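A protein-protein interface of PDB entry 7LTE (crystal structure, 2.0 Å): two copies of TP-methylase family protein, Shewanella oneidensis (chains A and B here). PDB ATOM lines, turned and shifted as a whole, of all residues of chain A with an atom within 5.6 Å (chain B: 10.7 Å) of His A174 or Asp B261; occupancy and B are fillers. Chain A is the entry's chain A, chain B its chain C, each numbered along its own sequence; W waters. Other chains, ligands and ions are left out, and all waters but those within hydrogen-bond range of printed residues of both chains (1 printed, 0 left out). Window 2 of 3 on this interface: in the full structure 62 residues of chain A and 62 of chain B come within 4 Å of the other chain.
Among the printed residues, pairs that only touch across the chains: His A174 with Asp B261, Thr A175 with Gly B263, Phe A152 with Tyr B247, Phe A152 with Leu B255, His A174 with Ile B257, His A174 with Leu B262, Leu A176 with Gly B263, Phe A152 with Leu B262 and Phe A152 with Leu B252.
No position is printed for both chains.
Of the 11 pairs that touch across the chains among the printed residues, none has its exchanged pair printed and touching as well.
The guanidinium group (NH2) of Arg A185 sits at hydrogen-bond distance from the backbone carbonyl oxygen (O) of Leu B255 (3.2 Å).
The backbone carbonyl oxygen (O) of His A174 sits at hydrogen-bond distance from the backbone NH (N) of Gly B263 (2.8 Å).
Water W1 bridges NH1 of Arg A185 (2.7 Å) and O of Lys B254 (2.8 Å).
Of the 7 printed residues of chain A, 5 touch a printed residue of chain B.
Of the 15 printed residues of chain B, 7 touch a printed residue of chain A.
Hydrophobic or aromatic side chains of chain B that line the printed part of chain A: Tyr B247, Leu B252, Leu B255, Ile B257 and Leu B262.
Among the printed residues, no Asp or Glu carboxylate lies within 4 Å of a Lys or Arg side-chain nitrogen of the other chain.
His A174 touches just these residues of chain B: Ile B257 (3.6 Å), Asp B261 (3.3 Å), Leu B262 (3.6 Å) and Gly B263 (2.8 Å).
Asp B261 touches one residue of chain A.
Gly A172 touches none of the printed residues of chain B.
No residue of chain B comes within 4 Å of Glu A173.
Thr A175 touches one residue of chain B.
Of the printed residues of chain B, Leu A176 touches Gly B263 (3.6 Å).
Printed residues of chain A within 4 Å of Gly B263: His A174 (2.8 Å), Thr A175 (3.5 Å) and Leu A176 (3.6 Å).
The nearest residue of chain B that does not touch His A174 is Leu B255 (5.8 Å).
The nearest printed residue of chain A that does not touch Ile B257 is Phe A152 (4.3 Å).
The backbone NH (N) of Gly B258 sits at hydrogen-bond distance from the side-chain carboxylate (OD2) of Asp B261.
The side-chain carboxylate (OE1) of Glu A173 sits at hydrogen-bond distance from the backbone NH (N) of Leu A176 (3.0 Å).
The backbone carbonyl oxygen of Leu B252 lies within hydrogen-bond range of the backbone NH of Ile B257 (2.9 Å).
OE2 of Glu A173 sits at hydrogen-bond distance from OG1 of Thr A175 (2.6 Å).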
ATOM      1  N   PHE A 152      14.896 -20.310 -21.933  1.00  0.00           N
ATOM      2  CA  PHE A 152      14.963 -19.740 -20.564  1.00  0.00           C
ATOM      3  C   PHE A 152      16.219 -20.180 -19.820  1.00  0.00           C
ATOM      4  O   PHE A 152      16.607 -19.458 -18.898  1.00  0.00           O
ATOM      5  CB  PHE A 152      13.731 -20.092 -19.725  1.00  0.00           C
ATOM      6  CG  PHE A 152      12.430 -19.582 -20.291  1.00  0.00           C
ATOM      7  CD1 PHE A 152      12.391 -18.540 -21.214  1.00  0.00           C
ATOM      8  CD2 PHE A 152      11.219 -20.182 -19.941  1.00  0.00           C
ATOM      9  CE1 PHE A 152      11.180 -18.091 -21.737  1.00  0.00           C
ATOM     10  CE2 PHE A 152      10.024 -19.756 -20.504  1.00  0.00           C
ATOM     11  CZ  PHE A 152       9.998 -18.730 -21.410  1.00  0.00           C
ATOM     12  N   GLY A 172       8.594 -19.828 -25.470  1.00  0.00           N
ATOM     13  CA  GLY A 172       8.944 -18.496 -24.967  1.00  0.00           C
ATOM     14  C   GLY A 172       7.805 -17.889 -24.173  1.00  0.00           C
ATOM     15  O   GLY A 172       7.977 -16.765 -23.721  1.00  0.00           O
ATOM     16  N   GLU A 173       6.703 -18.629 -24.001  1.00  0.00           N
ATOM     17  CA  GLU A 173       5.477 -18.176 -23.302  1.00  0.00           C
ATOM     18  C   GLU A 173       5.718 -18.391 -21.812  1.00  0.00           C
ATOM     19  O   GLU A 173       5.438 -19.494 -21.297  1.00  0.00           O
ATOM     20  CB  GLU A 173       4.241 -18.926 -23.788  1.00  0.00           C
ATOM     21  CG  GLU A 173       2.940 -18.211 -23.458  1.00  0.00           C
ATOM     22  CD  GLU A 173       2.727 -17.939 -21.967  1.00  0.00           C
ATOM     23  OE1 GLU A 173       2.217 -18.833 -21.269  1.00  0.00           O
ATOM     24  OE2 GLU A 173       3.111 -16.811 -21.505  1.00  0.00           O
ATOM     25  N   HIS A 174       6.233 -17.359 -21.157  1.00  0.00           N
ATOM     26  CA  HIS A 174       6.901 -17.462 -19.842  1.00  0.00           C
ATOM     27  C   HIS A 174       5.878 -17.580 -18.715  1.00  0.00           C
ATOM     28  O   HIS A 174       6.242 -18.021 -17.630  1.00  0.00           O
ATOM     29  CB  HIS A 174       7.887 -16.291 -19.672  1.00  0.00           C
ATOM     30  CG  HIS A 174       7.233 -14.957 -19.564  1.00  0.00           C
ATOM     31  ND1 HIS A 174       6.858 -14.244 -20.680  1.00  0.00           N
ATOM     32  CD2 HIS A 174       6.809 -14.251 -18.481  1.00  0.00           C
ATOM     33  CE1 HIS A 174       6.245 -13.137 -20.303  1.00  0.00           C
ATOM     34  NE2 HIS A 174       6.195 -13.122 -18.957  1.00  0.00           N
ATOM     35  N   THR A 175       4.631 -17.180 -18.954  1.00  0.00           N
ATOM     36  CA  THR A 175       3.625 -17.028 -17.878  1.00  0.00           C
ATOM     37  C   THR A 175       3.035 -18.400 -17.514  1.00  0.00           C
ATOM     38  O   THR A 175       2.530 -18.530 -16.381  1.00  0.00           O
ATOM     39  CB  THR A 175       2.551 -15.990 -18.244  1.00  0.00           C
ATOM     40  OG1 THR A 175       1.743 -16.516 -19.297  1.00  0.00           O
ATOM     41  CG2 THR A 175       3.158 -14.638 -18.622  1.00  0.00           C
ATOM     42  N   LEU A 176       3.033 -19.339 -18.468  1.00  0.00           N
ATOM     43  CA  LEU A 176       2.289 -20.627 -18.356  1.00  0.00           C
ATOM     44  C   LEU A 176       0.783 -20.343 -18.237  1.00  0.00           C
ATOM     45  O   LEU A 176       0.068 -21.185 -17.648  1.00  0.00           O
ATOM     46  CB  LEU A 176       2.785 -21.383 -17.130  1.00  0.00           C
ATOM     47  CG  LEU A 176       4.298 -21.580 -17.028  1.00  0.00           C
ATOM     48  CD1 LEU A 176       4.620 -22.472 -15.844  1.00  0.00           C
ATOM     49  CD2 LEU A 176       4.848 -22.204 -18.318  1.00  0.00           C
ATOM     50  N   ARG A 185       8.377 -14.007 -30.472  1.00  0.00           N
ATOM     51  CA  ARG A 185       9.059 -14.971 -29.556  1.00  0.00           C
ATOM     52  C   ARG A 185       9.741 -16.056 -30.395  1.00  0.00           C
ATOM     53  O   ARG A 185      10.877 -16.443 -30.087  1.00  0.00           O
ATOM     54  CB  ARG A 185       8.068 -15.599 -28.569  1.00  0.00           C
ATOM     55  CG  ARG A 185       7.448 -14.619 -27.580  1.00  0.00           C
ATOM     56  CD  ARG A 185       8.412 -14.328 -26.491  1.00  0.00           C
ATOM     57  NE  ARG A 185       7.940 -13.496 -25.388  1.00  0.00           N
ATOM     58  CZ  ARG A 185       8.162 -12.180 -25.234  1.00  0.00           C
ATOM     59  NH1 ARG A 185       8.752 -11.457 -26.185  1.00  0.00           N
ATOM     60  NH2 ARG A 185       7.736 -11.581 -24.131  1.00  0.00           N
ATOM     61  N   TYR B 247      19.895 -19.936 -15.554  1.00  0.00           N
ATOM     62  CA  TYR B 247      19.086 -18.977 -16.344  1.00  0.00           C
ATOM     63  C   TYR B 247      19.908 -18.506 -17.540  1.00  0.00           C
ATOM     64  O   TYR B 247      21.124 -18.176 -17.385  1.00  0.00           O
ATOM     65  CB  TYR B 247      18.554 -17.836 -15.481  1.00  0.00           C
ATOM     66  CG  TYR B 247      17.472 -18.275 -14.536  1.00  0.00           C
ATOM     67  CD1 TYR B 247      16.245 -18.715 -15.000  1.00  0.00           C
ATOM     68  CD2 TYR B 247      17.684 -18.250 -13.165  1.00  0.00           C
ATOM     69  CE1 TYR B 247      15.265 -19.148 -14.125  1.00  0.00           C
ATOM     70  CE2 TYR B 247      16.717 -18.680 -12.283  1.00  0.00           C
ATOM     71  CZ  TYR B 247      15.492 -19.106 -12.762  1.00  0.00           C
ATOM     72  OH  TYR B 247      14.488 -19.516 -11.934  1.00  0.00           O
ATOM     73  N   TYR B 249      20.188 -15.595 -19.210  1.00  0.00           N
ATOM     74  CA  TYR B 249      19.981 -14.130 -19.048  1.00  0.00           C
ATOM     75  C   TYR B 249      20.019 -13.427 -20.413  1.00  0.00           C
ATOM     76  O   TYR B 249      19.302 -12.441 -20.621  1.00  0.00           O
ATOM     77  CB  TYR B 249      20.995 -13.546 -18.056  1.00  0.00           C
ATOM     78  CG  TYR B 249      20.677 -13.851 -16.614  1.00  0.00           C
ATOM     79  CD1 TYR B 249      19.666 -13.173 -15.952  1.00  0.00           C
ATOM     80  CD2 TYR B 249      21.380 -14.801 -15.901  1.00  0.00           C
ATOM     81  CE1 TYR B 249      19.339 -13.443 -14.639  1.00  0.00           C
ATOM     82  CE2 TYR B 249      21.056 -15.111 -14.592  1.00  0.00           C
ATOM     83  CZ  TYR B 249      20.046 -14.418 -13.952  1.00  0.00           C
ATOM     84  OH  TYR B 249      19.691 -14.712 -12.665  1.00  0.00           O
ATOM     85  N   ILE B 251      18.864 -14.557 -23.367  1.00  0.00           N
ATOM     86  CA  ILE B 251      17.583 -14.740 -24.102  1.00  0.00           C
ATOM     87  C   ILE B 251      16.467 -14.077 -23.300  1.00  0.00           C
ATOM     88  O   ILE B 251      15.595 -13.429 -23.902  1.00  0.00           O
ATOM     89  CB  ILE B 251      17.353 -16.228 -24.375  1.00  0.00           C
ATOM     90  CG1 ILE B 251      18.508 -16.826 -25.191  1.00  0.00           C
ATOM     91  CG2 ILE B 251      15.997 -16.455 -25.054  1.00  0.00           C
ATOM     92  CD1 ILE B 251      18.623 -16.306 -26.595  1.00  0.00           C
ATOM     93  N   LEU B 252      16.532 -14.160 -21.974  1.00  0.00           N
ATOM     94  CA  LEU B 252      15.526 -13.498 -21.109  1.00  0.00           C
ATOM     95  C   LEU B 252      15.522 -12.007 -21.443  1.00  0.00           C
ATOM     96  O   LEU B 252      14.406 -11.437 -21.579  1.00  0.00           O
ATOM     97  CB  LEU B 252      15.830 -13.798 -19.643  1.00  0.00           C
ATOM     98  CG  LEU B 252      15.657 -15.263 -19.212  1.00  0.00           C
ATOM     99  CD1 LEU B 252      16.070 -15.462 -17.740  1.00  0.00           C
ATOM    100  CD2 LEU B 252      14.223 -15.704 -19.387  1.00  0.00           C
ATOM    101  N   ALA B 253      16.714 -11.428 -21.639  1.00  0.00           N
ATOM    102  CA  ALA B 253      16.940 -10.005 -21.971  1.00  0.00           C
ATOM    103  C   ALA B 253      16.265  -9.678 -23.294  1.00  0.00           C
ATOM    104  O   ALA B 253      15.559  -8.650 -23.353  1.00  0.00           O
ATOM    105  CB  ALA B 253      18.425  -9.703 -22.028  1.00  0.00           C
ATOM    106  N   LYS B 254      16.395 -10.542 -24.299  1.00  0.00           N
ATOM    107  CA  LYS B 254      15.719 -10.327 -25.615  1.00  0.00           C
ATOM    108  C   LYS B 254      14.179 -10.458 -25.485  1.00  0.00           C
ATOM    109  O   LYS B 254      13.427  -9.753 -26.226  1.00  0.00           O
ATOM    110  CB  LYS B 254      16.295 -11.303 -26.635  1.00  0.00           C
ATOM    111  CG  LYS B 254      17.667 -10.913 -27.159  1.00  0.00           C
ATOM    112  CD  LYS B 254      18.341 -11.974 -27.979  1.00  0.00           C
ATOM    113  CE  LYS B 254      19.845 -11.809 -28.075  1.00  0.00           C
ATOM    114  NZ  LYS B 254      20.234 -10.495 -28.643  1.00  0.00           N
ATOM    115  N   LEU B 255      13.701 -11.285 -24.563  1.00  0.00           N
ATOM    116  CA  LEU B 255      12.252 -11.496 -24.329  1.00  0.00           C
ATOM    117  C   LEU B 255      11.746 -10.371 -23.412  1.00  0.00           C
ATOM    118  O   LEU B 255      10.514 -10.324 -23.135  1.00  0.00           O
ATOM    119  CB  LEU B 255      12.041 -12.875 -23.686  1.00  0.00           C
ATOM    120  CG  LEU B 255      12.377 -14.088 -24.542  1.00  0.00           C
ATOM    121  CD1 LEU B 255      12.476 -15.358 -23.693  1.00  0.00           C
ATOM    122  CD2 LEU B 255      11.352 -14.277 -25.622  1.00  0.00           C
ATOM    123  N   GLY B 256      12.671  -9.551 -22.886  1.00  0.00           N
ATOM    124  CA  GLY B 256      12.363  -8.412 -22.011  1.00  0.00           C
ATOM    125  C   GLY B 256      11.839  -8.852 -20.659  1.00  0.00           C
ATOM    126  O   GLY B 256      11.079  -8.131 -20.081  1.00  0.00           O
ATOM    127  N   ILE B 257      12.284  -9.998 -20.145  1.00  0.00           N
ATOM    128  CA  ILE B 257      11.838 -10.541 -18.828  1.00  0.00           C
ATOM    129  C   ILE B 257      13.039 -10.927 -17.964  1.00  0.00           C
ATOM    130  O   ILE B 257      14.188 -10.977 -18.468  1.00  0.00           O
ATOM    131  CB  ILE B 257      10.911 -11.754 -19.054  1.00  0.00           C
ATOM    132  CG1 ILE B 257      11.600 -12.858 -19.867  1.00  0.00           C
ATOM    133  CG2 ILE B 257       9.609 -11.306 -19.688  1.00  0.00           C
ATOM    134  CD1 ILE B 257      10.799 -14.148 -19.965  1.00  0.00           C
ATOM    135  N   GLY B 258      12.769 -11.262 -16.699  1.00  0.00           N
ATOM    136  CA  GLY B 258      13.770 -11.857 -15.801  1.00  0.00           C
ATOM    137  C   GLY B 258      13.242 -13.144 -15.183  1.00  0.00           C
ATOM    138  O   GLY B 258      12.068 -13.495 -15.348  1.00  0.00           O
ATOM    139  N   PRO B 259      14.084 -13.874 -14.427  1.00  0.00           N
ATOM    140  CA  PRO B 259      13.651 -15.118 -13.799  1.00  0.00           C
ATOM    141  C   PRO B 259      12.416 -14.932 -12.893  1.00  0.00           C
ATOM    142  O   PRO B 259      11.579 -15.827 -12.827  1.00  0.00           O
ATOM    143  CB  PRO B 259      14.855 -15.537 -12.950  1.00  0.00           C
ATOM    144  CG  PRO B 259      16.041 -14.824 -13.563  1.00  0.00           C
ATOM    145  CD  PRO B 259      15.480 -13.537 -14.125  1.00  0.00           C
ATOM    146  N   GLU B 260      12.318 -13.780 -12.221  1.00  0.00           N
ATOM    147  CA  GLU B 260      11.173 -13.473 -11.313  1.00  0.00           C
ATOM    148  C   GLU B 260       9.845 -13.483 -12.091  1.00  0.00           C
ATOM    149  O   GLU B 260       8.815 -13.637 -11.450  1.00  0.00           O
ATOM    150  CB  GLU B 260      11.411 -12.146 -10.589  1.00  0.00           C
ATOM    151  CG  GLU B 260      11.397 -10.922 -11.503  1.00  0.00           C
ATOM    152  CD  GLU B 260      12.728 -10.497 -12.125  1.00  0.00           C
ATOM    153  OE1 GLU B 260      13.699 -11.313 -12.110  1.00  0.00           O
ATOM    154  OE2 GLU B 260      12.788  -9.343 -12.658  1.00  0.00           O
ATOM    155  N   ASP B 261       9.893 -13.317 -13.423  1.00  0.00           N
ATOM    156  CA  ASP B 261       8.711 -13.156 -14.307  1.00  0.00           C
ATOM    157  C   ASP B 261       8.177 -14.519 -14.741  1.00  0.00           C
ATOM    158  O   ASP B 261       7.014 -14.564 -15.180  1.00  0.00           O
ATOM    159  CB  ASP B 261       9.049 -12.324 -15.540  1.00  0.00           C
ATOM    160  CG  ASP B 261       9.293 -10.873 -15.205  1.00  0.00           C
ATOM    161  OD1 ASP B 261       8.527 -10.338 -14.381  1.00  0.00           O
ATOM    162  OD2 ASP B 261      10.266 -10.337 -15.708  1.00  0.00           O
ATOM    163  N   LEU B 262       8.984 -15.575 -14.637  1.00  0.00           N
ATOM    164  CA  LEU B 262       8.594 -16.939 -15.078  1.00  0.00           C
ATOM    165  C   LEU B 262       7.431 -17.445 -14.214  1.00  0.00           C
ATOM    166  O   LEU B 262       7.504 -17.282 -12.969  1.00  0.00           O
ATOM    167  CB  LEU B 262       9.804 -17.873 -14.947  1.00  0.00           C
ATOM    168  CG  LEU B 262      10.985 -17.536 -15.865  1.00  0.00           C
ATOM    169  CD1 LEU B 262      12.162 -18.439 -15.568  1.00  0.00           C
ATOM    170  CD2 LEU B 262      10.588 -17.649 -17.315  1.00  0.00           C
ATOM    171  N   GLY B 263       6.432 -18.068 -14.848  1.00  0.00           N
ATOM    172  CA  GLY B 263       5.290 -18.679 -14.158  1.00  0.00           C
ATOM    173  C   GLY B 263       5.696 -19.950 -13.410  1.00  0.00           C
ATOM    174  O   GLY B 263       4.925 -20.412 -12.544  1.00  0.00           O
ATOM    175  OXT GLY B 263       6.777 -20.542 -13.633  1.00  0.00           O
HETATM  176  O   HOH W   1      10.695  -9.716 -26.821  1.00  0.00           O
